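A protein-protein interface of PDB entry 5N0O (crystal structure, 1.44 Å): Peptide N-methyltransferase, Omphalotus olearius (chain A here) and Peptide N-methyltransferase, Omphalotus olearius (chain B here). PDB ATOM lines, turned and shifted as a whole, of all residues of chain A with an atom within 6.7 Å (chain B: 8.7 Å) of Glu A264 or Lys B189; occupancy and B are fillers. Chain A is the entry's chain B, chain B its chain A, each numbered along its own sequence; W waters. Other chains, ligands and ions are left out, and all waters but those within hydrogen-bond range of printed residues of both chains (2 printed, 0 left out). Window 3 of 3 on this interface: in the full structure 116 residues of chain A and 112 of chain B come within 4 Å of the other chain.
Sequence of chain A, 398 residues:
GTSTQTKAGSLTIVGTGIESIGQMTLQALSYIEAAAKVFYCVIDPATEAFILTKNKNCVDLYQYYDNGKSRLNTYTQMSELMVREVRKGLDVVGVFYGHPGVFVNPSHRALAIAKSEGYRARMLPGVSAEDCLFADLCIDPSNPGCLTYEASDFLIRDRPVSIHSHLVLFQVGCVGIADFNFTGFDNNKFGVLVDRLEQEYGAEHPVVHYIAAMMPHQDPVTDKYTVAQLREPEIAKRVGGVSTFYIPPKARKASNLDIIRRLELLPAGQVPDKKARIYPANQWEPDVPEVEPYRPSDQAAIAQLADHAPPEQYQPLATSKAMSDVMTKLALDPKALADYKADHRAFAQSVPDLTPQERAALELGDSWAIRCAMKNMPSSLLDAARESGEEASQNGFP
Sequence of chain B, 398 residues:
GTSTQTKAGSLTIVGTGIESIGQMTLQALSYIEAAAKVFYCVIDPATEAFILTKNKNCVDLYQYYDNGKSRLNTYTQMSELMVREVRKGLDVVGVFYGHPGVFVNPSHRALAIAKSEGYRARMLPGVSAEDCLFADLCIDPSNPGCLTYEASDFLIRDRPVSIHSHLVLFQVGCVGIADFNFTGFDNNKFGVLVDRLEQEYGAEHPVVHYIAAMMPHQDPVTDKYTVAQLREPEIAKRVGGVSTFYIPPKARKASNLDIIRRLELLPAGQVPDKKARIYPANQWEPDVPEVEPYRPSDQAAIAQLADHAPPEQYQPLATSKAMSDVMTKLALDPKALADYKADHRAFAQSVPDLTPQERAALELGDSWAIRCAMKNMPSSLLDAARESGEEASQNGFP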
ATOM      1  N   ILE A 259      24.482  21.778 -18.777  1.00  0.00           N
ATOM      2  CA  ILE A 259      25.064  22.741 -19.700  1.00  0.00           C
ATOM      3  C   ILE A 259      24.681  22.418 -21.158  1.00  0.00           C
ATOM      4  O   ILE A 259      24.325  23.328 -21.897  1.00  0.00           O
ATOM      5  CB  ILE A 259      26.603  22.856 -19.519  1.00  0.00           C
ATOM      6  CG1 ILE A 259      26.956  23.391 -18.106  1.00  0.00           C
ATOM      7  CG2 ILE A 259      27.219  23.725 -20.611  1.00  0.00           C
ATOM      8  CD1 ILE A 259      26.559  24.828 -17.811  1.00  0.00           C
ATOM      9  N   ILE A 260      24.730  21.151 -21.570  1.00  0.00           N
ATOM     10  CA  ILE A 260      24.249  20.771 -22.913  1.00  0.00           C
ATOM     11  C   ILE A 260      22.815  21.272 -23.154  1.00  0.00           C
ATOM     12  O   ILE A 260      22.528  21.823 -24.222  1.00  0.00           O
ATOM     13  CB  ILE A 260      24.343  19.240 -23.169  1.00  0.00           C
ATOM     14  CG1 ILE A 260      25.807  18.834 -23.375  1.00  0.00           C
ATOM     15  CG2 ILE A 260      23.530  18.825 -24.407  1.00  0.00           C
ATOM     16  CD1 ILE A 260      26.057  17.345 -23.283  1.00  0.00           C
ATOM     17  N   ARG A 261      21.935  21.097 -22.169  1.00  0.00           N
ATOM     18  CA  ARG A 261      20.551  21.594 -22.262  1.00  0.00           C
ATOM     19  C   ARG A 261      20.466  23.126 -22.301  1.00  0.00           C
ATOM     20  O   ARG A 261      19.777  23.676 -23.158  1.00  0.00           O
ATOM     21  CB  ARG A 261      19.683  21.064 -21.117  1.00  0.00           C
ATOM     22  CG  ARG A 261      18.194  21.405 -21.254  1.00  0.00           C
ATOM     23  CD  ARG A 261      17.360  20.980 -20.051  1.00  0.00           C
ATOM     24  NE  ARG A 261      18.019  21.285 -18.778  1.00  0.00           N
ATOM     25  CZ  ARG A 261      18.166  22.499 -18.235  1.00  0.00           C
ATOM     26  NH1 ARG A 261      17.685  23.601 -18.823  1.00  0.00           N
ATOM     27  NH2 ARG A 261      18.812  22.615 -17.077  1.00  0.00           N
ATOM     28  N   ARG A 262      21.159  23.815 -21.392  1.00  0.00           N
ATOM     29  CA  ARG A 262      21.101  25.290 -21.343  1.00  0.00           C
ATOM     30  C   ARG A 262      21.662  25.962 -22.607  1.00  0.00           C
ATOM     31  O   ARG A 262      21.177  27.026 -23.011  1.00  0.00           O
ATOM     32  CB  ARG A 262      21.834  25.838 -20.108  1.00  0.00           C
ATOM     33  CG  ARG A 262      21.116  25.602 -18.789  1.00  0.00           C
ATOM     34  CD  ARG A 262      21.780  26.373 -17.649  1.00  0.00           C
ATOM     35  NE  ARG A 262      21.428  27.800 -17.641  1.00  0.00           N
ATOM     36  CZ  ARG A 262      21.890  28.703 -16.768  1.00  0.00           C
ATOM     37  NH1 ARG A 262      22.745  28.360 -15.806  1.00  0.00           N
ATOM     38  NH2 ARG A 262      21.496  29.973 -16.862  1.00  0.00           N
ATOM     39  N   LEU A 263      22.672  25.342 -23.219  1.00  0.00           N
ATOM     40  CA  LEU A 263      23.263  25.844 -24.468  1.00  0.00           C
ATOM     41  C   LEU A 263      22.584  25.275 -25.725  1.00  0.00           C
ATOM     42  O   LEU A 263      22.965  25.624 -26.846  1.00  0.00           O
ATOM     43  CB  LEU A 263      24.776  25.574 -24.497  1.00  0.00           C
ATOM     44  CG  LEU A 263      25.630  26.244 -23.407  1.00  0.00           C
ATOM     45  CD1 LEU A 263      27.105  25.997 -23.677  1.00  0.00           C
ATOM     46  CD2 LEU A 263      25.360  27.736 -23.299  1.00  0.00           C
ATOM     47  N   GLU A 264      21.600  24.391 -25.545  1.00  0.00           N
ATOM     48  CA  GLU A 264      20.777  23.876 -26.656  1.00  0.00           C
ATOM     49  C   GLU A 264      21.628  23.141 -27.718  1.00  0.00           C
ATOM     50  O   GLU A 264      21.389  23.264 -28.928  1.00  0.00           O
ATOM     51  CB  GLU A 264      19.911  25.007 -27.254  1.00  0.00           C
ATOM     52  CG  GLU A 264      18.996  25.683 -26.233  1.00  0.00           C
ATOM     53  CD  GLU A 264      18.298  26.951 -26.728  1.00  0.00           C
ATOM     54  OE1 GLU A 264      18.592  27.434 -27.836  1.00  0.00           O
ATOM     55  OE2 GLU A 264      17.450  27.479 -25.980  1.00  0.00           O
ATOM     56  N   LEU A 265      22.570  22.326 -27.243  1.00  0.00           N
ATOM     57  CA  LEU A 265      23.569  21.650 -28.099  1.00  0.00           C
ATOM     58  C   LEU A 265      23.178  20.250 -28.604  1.00  0.00           C
ATOM     59  O   LEU A 265      23.810  19.727 -29.528  1.00  0.00           O
ATOM     60  CB  LEU A 265      24.911  21.539 -27.360  1.00  0.00           C
ATOM     61  CG  LEU A 265      25.571  22.842 -26.906  1.00  0.00           C
ATOM     62  CD1 LEU A 265      26.837  22.531 -26.116  1.00  0.00           C
ATOM     63  CD2 LEU A 265      25.877  23.741 -28.094  1.00  0.00           C
ATOM     64  N   LEU A 266      22.172  19.633 -27.988  1.00  0.00           N
ATOM     65  CA  LEU A 266      21.739  18.271 -28.354  1.00  0.00           C
ATOM     66  C   LEU A 266      20.279  18.119 -27.951  1.00  0.00           C
ATOM     67  O   LEU A 266      19.926  18.495 -26.831  1.00  0.00           O
ATOM     68  CB  LEU A 266      22.593  17.228 -27.609  1.00  0.00           C
ATOM     69  CG  LEU A 266      22.502  15.736 -27.961  1.00  0.00           C
ATOM     70  CD1 LEU A 266      23.061  15.488 -29.355  1.00  0.00           C
ATOM     71  CD2 LEU A 266      23.258  14.898 -26.933  1.00  0.00           C
ATOM     72  N   PRO A 267      19.416  17.571 -28.841  1.00  0.00           N
ATOM     73  CA  PRO A 267      18.051  17.275 -28.405  1.00  0.00           C
ATOM     74  C   PRO A 267      18.003  16.195 -27.327  1.00  0.00           C
ATOM     75  O   PRO A 267      18.912  15.353 -27.244  1.00  0.00           O
ATOM     76  CB  PRO A 267      17.360  16.761 -29.685  1.00  0.00           C
ATOM     77  CG  PRO A 267      18.191  17.267 -30.804  1.00  0.00           C
ATOM     78  CD  PRO A 267      19.597  17.311 -30.282  1.00  0.00           C
ATOM     79  N   ALA B 151      35.963  29.536 -23.624  1.00  0.00           N
ATOM     80  CA  ALA B 151      34.811  29.766 -22.722  1.00  0.00           C
ATOM     81  C   ALA B 151      33.683  28.712 -22.796  1.00  0.00           C
ATOM     82  O   ALA B 151      33.141  28.290 -21.757  1.00  0.00           O
ATOM     83  CB  ALA B 151      34.234  31.170 -22.929  1.00  0.00           C
ATOM     84  N   SER B 152      33.327  28.295 -24.009  1.00  0.00           N
ATOM     85  CA  SER B 152      32.276  27.275 -24.186  1.00  0.00           C
ATOM     86  C   SER B 152      32.737  25.901 -23.665  1.00  0.00           C
ATOM     87  O   SER B 152      32.001  25.243 -22.926  1.00  0.00           O
ATOM     88  CB  SER B 152      31.823  27.195 -25.647  1.00  0.00           C
ATOM     89  OG  SER B 152      31.217  28.415 -26.056  1.00  0.00           O
ATOM     90  N   LEU B 155      32.631  25.555 -19.882  1.00  0.00           N
ATOM     91  CA  LEU B 155      31.290  25.208 -19.396  1.00  0.00           C
ATOM     92  C   LEU B 155      30.876  23.770 -19.735  1.00  0.00           C
ATOM     93  O   LEU B 155      30.451  23.016 -18.845  1.00  0.00           O
ATOM     94  CB  LEU B 155      30.254  26.184 -19.959  1.00  0.00           C
ATOM     95  CG  LEU B 155      30.411  27.658 -19.577  1.00  0.00           C
ATOM     96  CD1 LEU B 155      29.426  28.509 -20.369  1.00  0.00           C
ATOM     97  CD2 LEU B 155      30.218  27.843 -18.076  1.00  0.00           C
ATOM     98  N   ILE B 156      30.991  23.389 -21.010  1.00  0.00           N
ATOM     99  CA  ILE B 156      30.455  22.089 -21.490  1.00  0.00           C
ATOM    100  C   ILE B 156      31.137  20.888 -20.808  1.00  0.00           C
ATOM    101  O   ILE B 156      30.460  19.930 -20.400  1.00  0.00           O
ATOM    102  CB  ILE B 156      30.555  21.949 -23.033  1.00  0.00           C
ATOM    103  CG1 ILE B 156      29.750  23.043 -23.739  1.00  0.00           C
ATOM    104  CG2 ILE B 156      30.052  20.583 -23.506  1.00  0.00           C
ATOM    105  CD1 ILE B 156      30.172  23.274 -25.176  1.00  0.00           C
ATOM    106  N   VAL B 172      34.796  34.530 -25.113  1.00  0.00           N
ATOM    107  CA  VAL B 172      33.678  34.893 -24.222  1.00  0.00           C
ATOM    108  C   VAL B 172      32.544  35.628 -24.970  1.00  0.00           C
ATOM    109  O   VAL B 172      31.423  35.730 -24.442  1.00  0.00           O
ATOM    110  CB  VAL B 172      34.148  35.730 -22.997  1.00  0.00           C
ATOM    111  CG1 VAL B 172      35.066  34.913 -22.091  1.00  0.00           C
ATOM    112  CG2 VAL B 172      34.846  37.022 -23.415  1.00  0.00           C
ATOM    113  N   GLY B 173      32.837  36.145 -26.169  1.00  0.00           N
ATOM    114  CA  GLY B 173      31.840  36.798 -27.022  1.00  0.00           C
ATOM    115  C   GLY B 173      30.956  35.897 -27.865  1.00  0.00           C
ATOM    116  O   GLY B 173      30.073  36.406 -28.568  1.00  0.00           O
ATOM    117  N   CYS B 174      31.165  34.578 -27.818  1.00  0.00           N
ATOM    118  CA  CYS B 174      30.377  33.640 -28.633  1.00  0.00           C
ATOM    119  C   CYS B 174      30.058  32.313 -27.920  1.00  0.00           C
ATOM    120  O   CYS B 174      30.202  31.221 -28.494  1.00  0.00           O
ATOM    121  CB  CYS B 174      31.074  33.402 -29.984  1.00  0.00           C
ATOM    122  SG  CYS B 174      32.753  32.735 -29.921  1.00  0.00           S
ATOM    123  N   VAL B 175      29.531  32.432 -26.703  1.00  0.00           N
ATOM    124  CA  VAL B 175      29.220  31.263 -25.863  1.00  0.00           C
ATOM    125  C   VAL B 175      28.149  30.368 -26.507  1.00  0.00           C
ATOM    126  O   VAL B 175      27.031  30.811 -26.746  1.00  0.00           O
ATOM    127  CB  VAL B 175      28.781  31.708 -24.444  1.00  0.00           C
ATOM    128  CG1 VAL B 175      28.387  30.505 -23.585  1.00  0.00           C
ATOM    129  CG2 VAL B 175      29.895  32.510 -23.765  1.00  0.00           C
ATOM    130  N   GLY B 176      28.514  29.116 -26.791  1.00  0.00           N
ATOM    131  CA  GLY B 176      27.596  28.153 -27.412  1.00  0.00           C
ATOM    132  C   GLY B 176      27.259  28.352 -28.887  1.00  0.00           C
ATOM    133  O   GLY B 176      26.350  27.682 -29.393  1.00  0.00           O
ATOM    134  N   ILE B 177      27.978  29.240 -29.581  1.00  0.00           N
ATOM    135  CA  ILE B 177      27.639  29.624 -30.968  1.00  0.00           C
ATOM    136  C   ILE B 177      28.575  28.937 -31.965  1.00  0.00           C
ATOM    137  O   ILE B 177      29.794  29.088 -31.875  1.00  0.00           O
ATOM    138  CB  ILE B 177      27.719  31.155 -31.175  1.00  0.00           C
ATOM    139  CG1 ILE B 177      26.716  31.872 -30.266  1.00  0.00           C
ATOM    140  CG2 ILE B 177      27.451  31.513 -32.638  1.00  0.00           C
ATOM    141  CD1 ILE B 177      26.852  33.378 -30.245  1.00  0.00           C
ATOM    142  N   ASP B 186      25.159  37.431 -31.744  1.00  0.00           N
ATOM    143  CA  ASP B 186      24.088  37.629 -30.758  1.00  0.00           C
ATOM    144  C   ASP B 186      24.376  36.667 -29.590  1.00  0.00           C
ATOM    145  O   ASP B 186      23.954  35.506 -29.601  1.00  0.00           O
ATOM    146  CB  ASP B 186      22.706  37.357 -31.389  1.00  0.00           C
ATOM    147  CG  ASP B 186      21.550  37.432 -30.382  1.00  0.00           C
ATOM    148  OD1 ASP B 186      21.705  38.008 -29.283  1.00  0.00           O
ATOM    149  OD2 ASP B 186      20.464  36.905 -30.704  1.00  0.00           O
ATOM    150  N   ASN B 187      25.084  37.178 -28.582  1.00  0.00           N
ATOM    151  CA  ASN B 187      25.683  36.369 -27.509  1.00  0.00           C
ATOM    152  C   ASN B 187      24.685  36.104 -26.366  1.00  0.00           C
ATOM    153  O   ASN B 187      24.968  36.361 -25.189  1.00  0.00           O
ATOM    154  CB  ASN B 187      26.943  37.113 -27.010  1.00  0.00           C
ATOM    155  CG  ASN B 187      27.905  36.235 -26.215  1.00  0.00           C
ATOM    156  OD1 ASN B 187      27.936  35.010 -26.357  1.00  0.00           O
ATOM    157  ND2 ASN B 187      28.731  36.885 -25.390  1.00  0.00           N
ATOM    158  N   ASN B 188      23.531  35.539 -26.716  1.00  0.00           N
ATOM    159  CA  ASN B 188      22.412  35.412 -25.768  1.00  0.00           C
ATOM    160  C   ASN B 188      22.530  34.274 -24.728  1.00  0.00           C
ATOM    161  O   ASN B 188      21.661  34.164 -23.859  1.00  0.00           O
ATOM    162  CB  ASN B 188      21.050  35.368 -26.504  1.00  0.00           C
ATOM    163  CG  ASN B 188      20.915  34.202 -27.469  1.00  0.00           C
ATOM    164  OD1 ASN B 188      21.413  33.103 -27.235  1.00  0.00           O
ATOM    165  ND2 ASN B 188      20.206  34.443 -28.567  1.00  0.00           N
ATOM    166  N   LYS B 189      23.585  33.451 -24.801  1.00  0.00           N
ATOM    167  CA  LYS B 189      23.885  32.450 -23.764  1.00  0.00           C
ATOM    168  C   LYS B 189      25.013  32.895 -22.807  1.00  0.00           C
ATOM    169  O   LYS B 189      25.444  32.109 -21.946  1.00  0.00           O
ATOM    170  CB  LYS B 189      24.247  31.099 -24.400  1.00  0.00           C
ATOM    171  CG  LYS B 189      23.183  30.517 -25.328  1.00  0.00           C
ATOM    172  CD  LYS B 189      21.910  30.157 -24.588  1.00  0.00           C
ATOM    173  CE  LYS B 189      20.958  29.317 -25.440  1.00  0.00           C
ATOM    174  NZ  LYS B 189      20.429  30.042 -26.620  1.00  0.00           N
ATOM    175  N   PHE B 190      25.459  34.146 -22.938  1.00  0.00           N
ATOM    176  CA  PHE B 190      26.483  34.728 -22.050  1.00  0.00           C
ATOM    177  C   PHE B 190      26.133  34.585 -20.558  1.00  0.00           C
ATOM    178  O   PHE B 190      27.014  34.341 -19.733  1.00  0.00           O
ATOM    179  CB  PHE B 190      26.716  36.203 -22.438  1.00  0.00           C
ATOM    180  CG  PHE B 190      27.769  36.921 -21.613  1.00  0.00           C
ATOM    181  CD1 PHE B 190      29.112  36.603 -21.741  1.00  0.00           C
ATOM    182  CD2 PHE B 190      27.411  37.941 -20.737  1.00  0.00           C
ATOM    183  CE1 PHE B 190      30.075  37.280 -20.998  1.00  0.00           C
ATOM    184  CE2 PHE B 190      28.365  38.616 -19.995  1.00  0.00           C
ATOM    185  CZ  PHE B 190      29.697  38.286 -20.125  1.00  0.00           C
ATOM    186  N   GLY B 191      24.850  34.694 -20.212  1.00  0.00           N
ATOM    187  CA  GLY B 191      24.411  34.542 -18.820  1.00  0.00           C
ATOM    188  C   GLY B 191      24.736  33.203 -18.167  1.00  0.00           C
ATOM    189  O   GLY B 191      24.856  33.130 -16.939  1.00  0.00           O
ATOM    190  N   VAL B 192      24.866  32.154 -18.981  1.00  0.00           N
ATOM    191  CA  VAL B 192      25.280  30.826 -18.503  1.00  0.00           C
ATOM    192  C   VAL B 192      26.734  30.870 -17.998  1.00  0.00           C
ATOM    193  O   VAL B 192      27.063  30.267 -16.964  1.00  0.00           O
ATOM    194  CB  VAL B 192      25.106  29.730 -19.592  1.00  0.00           C
ATOM    195  CG1 VAL B 192      25.479  28.362 -19.042  1.00  0.00           C
ATOM    196  CG2 VAL B 192      23.669  29.716 -20.131  1.00  0.00           C
ATOM    197  N   LEU B 193      27.605  31.582 -18.718  1.00  0.00           N
ATOM    198  CA  LEU B 193      28.991  31.795 -18.242  1.00  0.00           C
ATOM    199  C   LEU B 193      29.024  32.594 -16.936  1.00  0.00           C
ATOM    200  O   LEU B 193      29.770  32.243 -15.998  1.00  0.00           O
ATOM    201  CB  LEU B 193      29.848  32.487 -19.308  1.00  0.00           C
ATOM    202  CG  LEU B 193      31.300  32.807 -18.926  1.00  0.00           C
ATOM    203  CD1 LEU B 193      32.104  31.551 -18.602  1.00  0.00           C
ATOM    204  CD2 LEU B 193      31.997  33.615 -20.016  1.00  0.00           C
ATOM    205  N   VAL B 194      28.200  33.642 -16.849  1.00  0.00           N
ATOM    206  CA  VAL B 194      28.172  34.485 -15.634  1.00  0.00           C
ATOM    207  C   VAL B 194      27.737  33.670 -14.396  1.00  0.00           C
ATOM    208  O   VAL B 194      28.326  33.826 -13.314  1.00  0.00           O
ATOM    209  CB  VAL B 194      27.286  35.742 -15.813  1.00  0.00           C
ATOM    210  CG1 VAL B 194      27.287  36.592 -14.543  1.00  0.00           C
ATOM    211  CG2 VAL B 194      27.767  36.573 -17.007  1.00  0.00           C
ATOM    212  N   ASP B 195      26.735  32.795 -14.556  1.00  0.00           N
ATOM    213  CA  ASP B 195      26.310  31.893 -13.462  1.00  0.00           C
ATOM    214  C   ASP B 195      27.461  31.017 -12.954  1.00  0.00           C
ATOM    215  O   ASP B 195      27.640  30.895 -11.745  1.00  0.00           O
ATOM    216  CB  ASP B 195      25.129  30.995 -13.880  1.00  0.00           C
ATOM    217  CG  ASP B 195      23.783  31.717 -13.880  1.00  0.00           C
ATOM    218  OD1 ASP B 195      23.665  32.867 -13.394  1.00  0.00           O
ATOM    219  OD2 ASP B 195      22.812  31.091 -14.354  1.00  0.00           O
HETATM  220  O   HOH W   1      21.303  33.189 -16.130  1.00  0.00           O
HETATM  221  O   HOH W   2      24.005  27.868 -27.851  1.00  0.00           O
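NH2 of Arg A262 lies within salt-bridge range of OD2 of Asp B195, at 3.0 Å. The side-chain amino group of Lys B189 lies within salt-bridge range of the side-chain carboxylate of Glu A264 (3.4 Å).
OD1 of Asn B188 is in hydrogen-bond range of NZ of Lys B189, at 3.3 Å. The backbone carbonyl oxygen (O) of Ile A260 is in hydrogen-bond range of the backbone NH (N) of Leu A265, at 3.1 Å.
Among the printed residues, merely in contact across the chains: Ile A259 with Leu B155, Ile A259 with Ile B156, Ile A259 with Val B192, Arg A262 with Lys B189, Arg A262 with Val B192, Leu A263 with Ile B156, Leu A263 with Lys B189 and Leu A265 with Ile B156.
Printed residues of chain B within 4 Å of Arg A262: Lys B189, Val B192 and Asp B195. Of the printed residues of chain A, Ile B156 touches Ile A259 (3.7 Å), Leu A263 (3.97 Å) and Leu A265 (3.5 Å). Of chain A, only Arg A262, Leu A263 and Glu A264 come within 4 Å of Lys B189. Printed residues of chain A within 4 Å of Val B192: Ile A259 and Arg A262. The nearest residue of chain B that does not touch Glu A264 is Asn B188 (6.4 Å). The nearest residue of chain A that does not touch Lys B189 is Arg A261 (6.2 Å).
Printed residues of chain B that touch a printed residue of chain A: Leu B155, Ile B156, Lys B189, Val B192 and Asp B195. Among the printed residues, Asp or Glu carboxylates within 4 Å of a Lys or Arg side-chain nitrogen of the other chain: Arg A262 with Asp B195 (3.0 Å) and Glu A264 with Lys B189 (3.4 Å).
Water W2 lies within hydrogen-bond range of O of Leu A263 (2.7 Å) and O of Gly B176 (2.8 Å). Water W1 lies within hydrogen-bond range of the side-chain carboxylate of Asp B195 and the guanidinium group of Arg A262.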
